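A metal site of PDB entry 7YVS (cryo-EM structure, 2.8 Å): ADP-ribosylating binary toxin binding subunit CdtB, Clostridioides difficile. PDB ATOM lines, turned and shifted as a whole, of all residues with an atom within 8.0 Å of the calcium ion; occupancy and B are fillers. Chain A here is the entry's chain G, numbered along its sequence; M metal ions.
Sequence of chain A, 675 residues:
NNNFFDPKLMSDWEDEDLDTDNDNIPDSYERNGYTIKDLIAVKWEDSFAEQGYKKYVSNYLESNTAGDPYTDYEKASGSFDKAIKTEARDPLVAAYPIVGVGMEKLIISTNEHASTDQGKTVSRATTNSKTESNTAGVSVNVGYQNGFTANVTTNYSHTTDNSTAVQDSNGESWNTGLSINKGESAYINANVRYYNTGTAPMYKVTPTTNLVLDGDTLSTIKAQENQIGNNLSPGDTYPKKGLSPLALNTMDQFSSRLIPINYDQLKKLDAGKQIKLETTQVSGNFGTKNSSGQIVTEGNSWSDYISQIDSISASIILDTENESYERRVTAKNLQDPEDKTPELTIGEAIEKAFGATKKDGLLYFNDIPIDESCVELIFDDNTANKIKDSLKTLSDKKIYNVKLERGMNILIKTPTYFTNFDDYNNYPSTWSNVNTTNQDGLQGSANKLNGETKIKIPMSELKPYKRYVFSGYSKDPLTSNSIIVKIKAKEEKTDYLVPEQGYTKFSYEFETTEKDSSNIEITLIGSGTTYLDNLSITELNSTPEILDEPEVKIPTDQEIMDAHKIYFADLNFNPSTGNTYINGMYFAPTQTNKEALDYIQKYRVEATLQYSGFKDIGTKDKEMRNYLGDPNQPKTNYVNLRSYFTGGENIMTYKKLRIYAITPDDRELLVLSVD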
ATOM      1  N   SER A 373     -15.920 -14.228  -0.876  1.00  0.00           N
ATOM      2  CA  SER A 373     -14.940 -14.419   0.181  1.00  0.00           C
ATOM      3  C   SER A 373     -15.134 -13.454   1.347  1.00  0.00           C
ATOM      4  O   SER A 373     -14.416 -13.573   2.342  1.00  0.00           O
ATOM      5  CB  SER A 373     -13.526 -14.265  -0.377  1.00  0.00           C
ATOM      6  OG  SER A 373     -13.264 -12.916  -0.702  1.00  0.00           O
ATOM      7  N   CYS A 374     -16.065 -12.520   1.239  1.00  0.00           N
ATOM      8  CA  CYS A 374     -16.285 -11.510   2.267  1.00  0.00           C
ATOM      9  C   CYS A 374     -17.669 -11.576   2.896  1.00  0.00           C
ATOM     10  O   CYS A 374     -17.988 -10.737   3.747  1.00  0.00           O
ATOM     11  CB  CYS A 374     -16.050 -10.113   1.697  1.00  0.00           C
ATOM     12  SG  CYS A 374     -14.541  -9.925   0.725  1.00  0.00           S
ATOM     13  N   PHE A 418     -15.478  -7.108   9.771  1.00  0.00           N
ATOM     14  CA  PHE A 418     -14.722  -7.780   8.733  1.00  0.00           C
ATOM     15  C   PHE A 418     -13.450  -6.987   8.453  1.00  0.00           C
ATOM     16  O   PHE A 418     -13.471  -5.754   8.515  1.00  0.00           O
ATOM     17  CB  PHE A 418     -15.554  -7.934   7.454  1.00  0.00           C
ATOM     18  CG  PHE A 418     -14.805  -8.523   6.305  1.00  0.00           C
ATOM     19  CD1 PHE A 418     -14.565  -9.886   6.235  1.00  0.00           C
ATOM     20  CD2 PHE A 418     -14.340  -7.714   5.277  1.00  0.00           C
ATOM     21  CE1 PHE A 418     -13.876 -10.429   5.174  1.00  0.00           C
ATOM     22  CE2 PHE A 418     -13.660  -8.257   4.213  1.00  0.00           C
ATOM     23  CZ  PHE A 418     -13.431  -9.613   4.167  1.00  0.00           C
ATOM     24  N   THR A 419     -12.367  -7.695   8.153  1.00  0.00           N
ATOM     25  CA  THR A 419     -11.120  -7.068   7.750  1.00  0.00           C
ATOM     26  C   THR A 419     -10.409  -7.953   6.735  1.00  0.00           C
ATOM     27  O   THR A 419     -10.416  -9.186   6.854  1.00  0.00           O
ATOM     28  CB  THR A 419     -10.206  -6.791   8.958  1.00  0.00           C
ATOM     29  OG1 THR A 419      -9.066  -6.033   8.529  1.00  0.00           O
ATOM     30  CG2 THR A 419      -9.737  -8.096   9.608  1.00  0.00           C
ATOM     31  N   ASN A 420      -9.813  -7.318   5.740  1.00  0.00           N
ATOM     32  CA  ASN A 420      -9.046  -8.011   4.707  1.00  0.00           C
ATOM     33  C   ASN A 420      -7.605  -7.543   4.641  1.00  0.00           C
ATOM     34  O   ASN A 420      -6.869  -7.977   3.739  1.00  0.00           O
ATOM     35  CB  ASN A 420      -9.721  -7.835   3.341  1.00  0.00           C
ATOM     36  CG  ASN A 420      -9.729  -6.397   2.888  1.00  0.00           C
ATOM     37  OD1 ASN A 420      -9.864  -5.478   3.693  1.00  0.00           O
ATOM     38  ND2 ASN A 420      -9.580  -6.192   1.586  1.00  0.00           N
ATOM     39  N   PHE A 421      -7.182  -6.668   5.543  1.00  0.00           N
ATOM     40  CA  PHE A 421      -5.798  -6.206   5.679  1.00  0.00           C
ATOM     41  C   PHE A 421      -5.326  -5.404   4.471  1.00  0.00           C
ATOM     42  O   PHE A 421      -4.115  -5.212   4.281  1.00  0.00           O
ATOM     43  CB  PHE A 421      -4.850  -7.384   5.933  1.00  0.00           C
ATOM     44  CG  PHE A 421      -5.404  -8.403   6.875  1.00  0.00           C
ATOM     45  CD1 PHE A 421      -5.843  -8.044   8.136  1.00  0.00           C
ATOM     46  CD2 PHE A 421      -5.490  -9.738   6.505  1.00  0.00           C
ATOM     47  CE1 PHE A 421      -6.353  -8.984   9.005  1.00  0.00           C
ATOM     48  CE2 PHE A 421      -6.000 -10.678   7.374  1.00  0.00           C
ATOM     49  CZ  PHE A 421      -6.427 -10.300   8.626  1.00  0.00           C
ATOM     50  N   ASP A 422      -6.244  -4.922   3.631  1.00  0.00           N
ATOM     51  CA  ASP A 422      -5.883  -3.965   2.589  1.00  0.00           C
ATOM     52  C   ASP A 422      -6.584  -2.628   2.770  1.00  0.00           C
ATOM     53  O   ASP A 422      -5.902  -1.602   2.926  1.00  0.00           O
ATOM     54  CB  ASP A 422      -6.217  -4.539   1.203  1.00  0.00           C
ATOM     55  CG  ASP A 422      -5.307  -5.666   0.804  1.00  0.00           C
ATOM     56  OD1 ASP A 422      -4.113  -5.625   1.157  1.00  0.00           O
ATOM     57  OD2 ASP A 422      -5.787  -6.610   0.143  1.00  0.00           O
ATOM     58  N   ASP A 423      -7.913  -2.607   2.774  1.00  0.00           N
ATOM     59  CA  ASP A 423      -8.665  -1.357   2.747  1.00  0.00           C
ATOM     60  C   ASP A 423      -9.832  -1.312   3.703  1.00  0.00           C
ATOM     61  O   ASP A 423     -10.325  -0.212   3.981  1.00  0.00           O
ATOM     62  CB  ASP A 423      -9.186  -1.094   1.328  1.00  0.00           C
ATOM     63  CG  ASP A 423      -8.075  -0.943   0.305  1.00  0.00           C
ATOM     64  OD1 ASP A 423      -6.998  -0.427   0.664  1.00  0.00           O
ATOM     65  OD2 ASP A 423      -8.274  -1.346  -0.856  1.00  0.00           O
ATOM     66  N   TYR A 424     -10.303  -2.450   4.214  1.00  0.00           N
ATOM     67  CA  TYR A 424     -11.565  -2.518   4.944  1.00  0.00           C
ATOM     68  C   TYR A 424     -11.309  -2.978   6.366  1.00  0.00           C
ATOM     69  O   TYR A 424     -10.578  -3.958   6.582  1.00  0.00           O
ATOM     70  CB  TYR A 424     -12.544  -3.449   4.236  1.00  0.00           C
ATOM     71  CG  TYR A 424     -13.979  -3.292   4.671  1.00  0.00           C
ATOM     72  CD1 TYR A 424     -14.726  -2.213   4.230  1.00  0.00           C
ATOM     73  CD2 TYR A 424     -14.574  -4.217   5.507  1.00  0.00           C
ATOM     74  CE1 TYR A 424     -16.033  -2.056   4.615  1.00  0.00           C
ATOM     75  CE2 TYR A 424     -15.891  -4.074   5.893  1.00  0.00           C
ATOM     76  CZ  TYR A 424     -16.617  -2.988   5.450  1.00  0.00           C
ATOM     77  OH  TYR A 424     -17.924  -2.831   5.835  1.00  0.00           O
ATOM     78  N   ASP A 440       0.119 -12.014   0.235  1.00  0.00           N
ATOM     79  CA  ASP A 440      -0.403 -13.377   0.319  1.00  0.00           C
ATOM     80  C   ASP A 440      -1.910 -13.275   0.485  1.00  0.00           C
ATOM     81  O   ASP A 440      -2.505 -12.221   0.237  1.00  0.00           O
ATOM     82  CB  ASP A 440       0.282 -14.147   1.457  1.00  0.00           C
ATOM     83  CG  ASP A 440       1.720 -14.504   1.139  1.00  0.00           C
ATOM     84  OD1 ASP A 440       1.930 -15.347   0.236  1.00  0.00           O
ATOM     85  OD2 ASP A 440       2.626 -13.961   1.787  1.00  0.00           O
ATOM     86  N   GLY A 441      -2.536 -14.360   0.912  1.00  0.00           N
ATOM     87  CA  GLY A 441      -3.963 -14.331   1.137  1.00  0.00           C
ATOM     88  C   GLY A 441      -4.743 -14.374  -0.159  1.00  0.00           C
ATOM     89  O   GLY A 441      -4.210 -14.543  -1.260  1.00  0.00           O
ATOM     90  N   LEU A 442      -6.061 -14.207  -0.024  1.00  0.00           N
ATOM     91  CA  LEU A 442      -6.930 -14.210  -1.185  1.00  0.00           C
ATOM     92  C   LEU A 442      -6.607 -13.053  -2.119  1.00  0.00           C
ATOM     93  O   LEU A 442      -6.542 -13.234  -3.341  1.00  0.00           O
ATOM     94  CB  LEU A 442      -8.398 -14.164  -0.750  1.00  0.00           C
ATOM     95  CG  LEU A 442      -9.096 -15.494  -0.471  1.00  0.00           C
ATOM     96  CD1 LEU A 442      -9.105 -16.364  -1.715  1.00  0.00           C
ATOM     97  CD2 LEU A 442      -8.462 -16.227   0.705  1.00  0.00           C
ATOM     98  N   GLN A 443      -6.408 -11.850  -1.568  1.00  0.00           N
ATOM     99  CA  GLN A 443      -6.060 -10.675  -2.376  1.00  0.00           C
ATOM    100  C   GLN A 443      -4.921  -9.925  -1.676  1.00  0.00           C
ATOM    101  O   GLN A 443      -5.166  -8.975  -0.929  1.00  0.00           O
ATOM    102  CB  GLN A 443      -7.275  -9.774  -2.576  1.00  0.00           C
ATOM    103  CG  GLN A 443      -8.554 -10.495  -2.950  1.00  0.00           C
ATOM    104  CD  GLN A 443      -9.475 -10.714  -1.768  1.00  0.00           C
ATOM    105  OE1 GLN A 443      -9.334 -10.065  -0.731  1.00  0.00           O
ATOM    106  NE2 GLN A 443     -10.428 -11.621  -1.917  1.00  0.00           N
ATOM    107  N   GLY A 444      -3.691 -10.347  -1.947  1.00  0.00           N
ATOM    108  CA  GLY A 444      -2.503  -9.571  -1.598  1.00  0.00           C
ATOM    109  C   GLY A 444      -2.418  -9.097  -0.163  1.00  0.00           C
ATOM    110  O   GLY A 444      -1.956  -7.985   0.096  1.00  0.00           O
ATOM    111  N   SER A 445      -2.837  -9.934   0.782  1.00  0.00           N
ATOM    112  CA  SER A 445      -2.830  -9.548   2.190  1.00  0.00           C
ATOM    113  C   SER A 445      -2.980 -10.777   3.084  1.00  0.00           C
ATOM    114  O   SER A 445      -3.891 -11.583   2.886  1.00  0.00           O
ATOM    115  CB  SER A 445      -3.963  -8.552   2.475  1.00  0.00           C
ATOM    116  OG  SER A 445      -5.213  -9.216   2.560  1.00  0.00           O
ATOM    117  N   ALA A 446      -2.077 -10.926   4.054  1.00  0.00           N
ATOM    118  CA  ALA A 446      -2.141 -12.068   4.955  1.00  0.00           C
ATOM    119  C   ALA A 446      -2.327 -11.664   6.412  1.00  0.00           C
ATOM    120  O   ALA A 446      -3.254 -12.165   7.068  1.00  0.00           O
ATOM    121  CB  ALA A 446      -0.862 -12.911   4.816  1.00  0.00           C
ATOM    122  N   ASN A 447      -1.486 -10.788   6.935  1.00  0.00           N
ATOM    123  CA  ASN A 447      -1.491 -10.393   8.343  1.00  0.00           C
ATOM    124  C   ASN A 447      -1.413 -11.618   9.259  1.00  0.00           C
ATOM    125  O   ASN A 447      -2.328 -11.932  10.009  1.00  0.00           O
ATOM    126  CB  ASN A 447      -2.708  -9.534   8.679  1.00  0.00           C
ATOM    127  CG  ASN A 447      -2.638  -8.931  10.071  1.00  0.00           C
ATOM    128  OD1 ASN A 447      -1.703  -9.197  10.822  1.00  0.00           O
ATOM    129  ND2 ASN A 447      -3.631  -8.122  10.422  1.00  0.00           N
ATOM    130  N   LEU A 532      -3.219 -16.235   7.085  1.00  0.00           N
ATOM    131  CA  LEU A 532      -4.620 -15.908   7.316  1.00  0.00           C
ATOM    132  C   LEU A 532      -5.104 -14.892   6.300  1.00  0.00           C
ATOM    133  O   LEU A 532      -4.315 -14.278   5.587  1.00  0.00           O
ATOM    134  CB  LEU A 532      -4.864 -15.348   8.720  1.00  0.00           C
ATOM    135  CG  LEU A 532      -4.578 -16.202   9.960  1.00  0.00           C
ATOM    136  CD1 LEU A 532      -4.566 -15.288  11.158  1.00  0.00           C
ATOM    137  CD2 LEU A 532      -5.630 -17.293  10.129  1.00  0.00           C
ATOM    138  N   ASP A 533      -6.435 -14.711   6.248  1.00  0.00           N
ATOM    139  CA  ASP A 533      -7.072 -13.654   5.475  1.00  0.00           C
ATOM    140  C   ASP A 533      -8.563 -13.634   5.780  1.00  0.00           C
ATOM    141  O   ASP A 533      -9.158 -14.669   6.090  1.00  0.00           O
ATOM    142  CB  ASP A 533      -6.860 -13.832   3.960  1.00  0.00           C
ATOM    143  CG  ASP A 533      -6.703 -12.515   3.248  1.00  0.00           C
ATOM    144  OD1 ASP A 533      -6.803 -11.464   3.909  1.00  0.00           O
ATOM    145  OD2 ASP A 533      -6.489 -12.518   2.020  1.00  0.00           O
ATOM    146  N   ASN A 534      -9.147 -12.448   5.669  1.00  0.00           N
ATOM    147  CA  ASN A 534     -10.605 -12.241   5.659  1.00  0.00           C
ATOM    148  C   ASN A 534     -11.267 -12.810   6.917  1.00  0.00           C
ATOM    149  O   ASN A 534     -12.069 -13.741   6.855  1.00  0.00           O
ATOM    150  CB  ASN A 534     -11.219 -12.840   4.389  1.00  0.00           C
ATOM    151  CG  ASN A 534     -10.748 -12.159   3.126  1.00  0.00           C
ATOM    152  OD1 ASN A 534     -10.376 -10.990   3.134  1.00  0.00           O
ATOM    153  ND2 ASN A 534     -10.761 -12.893   2.027  1.00  0.00           N
ATOM    154  N   LEU A 535     -10.933 -12.213   8.052  1.00  0.00           N
ATOM    155  CA  LEU A 535     -11.544 -12.585   9.329  1.00  0.00           C
ATOM    156  C   LEU A 535     -12.827 -11.801   9.518  1.00  0.00           C
ATOM    157  O   LEU A 535     -12.829 -10.569   9.396  1.00  0.00           O
ATOM    158  CB  LEU A 535     -10.588 -12.333  10.491  1.00  0.00           C
ATOM    159  CG  LEU A 535      -9.223 -13.016  10.398  1.00  0.00           C
ATOM    160  CD1 LEU A 535      -8.313 -12.516  11.513  1.00  0.00           C
ATOM    161  CD2 LEU A 535      -9.364 -14.525  10.451  1.00  0.00           C
HETATM  162 CA    CA M   1      -7.485  -9.831   2.221  1.00  0.00          CA
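The side-chain hydroxyl (OG) of Ser 445 sits close to the backbone carbonyl oxygen (O) of Gln 443, 3.5 Å away.
The side-chain carboxylate of Asp 533 lies close to the backbone NH of Leu 442, 2.7 Å away.
The backbone NH of Tyr 424 lies within hydrogen-bond range of the side-chain amide oxygen of Asn 420 (3.1 Å).
The backbone carbonyl oxygen of Gln 443 lies close to the side-chain carboxylate of Asp 422, 2.7 Å away.
The side-chain amide nitrogen (NE2) of Gln 443 lies within hydrogen-bond range of the side-chain hydroxyl (OG) of Ser 373.
Gln 443 touches the calcium ion (OE1 to CA, 3.5 Å).
Asn 534 touches the calcium ion.
Five residues have an atom within 4 Å of the calcium ion: Asn 420, Gln 443, Ser 445, Asp 533 and Asn 534.
Along chain A the residues within 4 Å of the calcium ion span positions 420 to 534.
The nearest printed residue that does not touch the calcium ion is Asp 422 (4.2 Å).
The calcium ion is bound by OG of Ser 445 (2.4 Å), OD1 of Asp 533 (2.4 Å), O of Asn 420 (2.5 Å) and OD2 of Asp 533 (2.9 Å).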
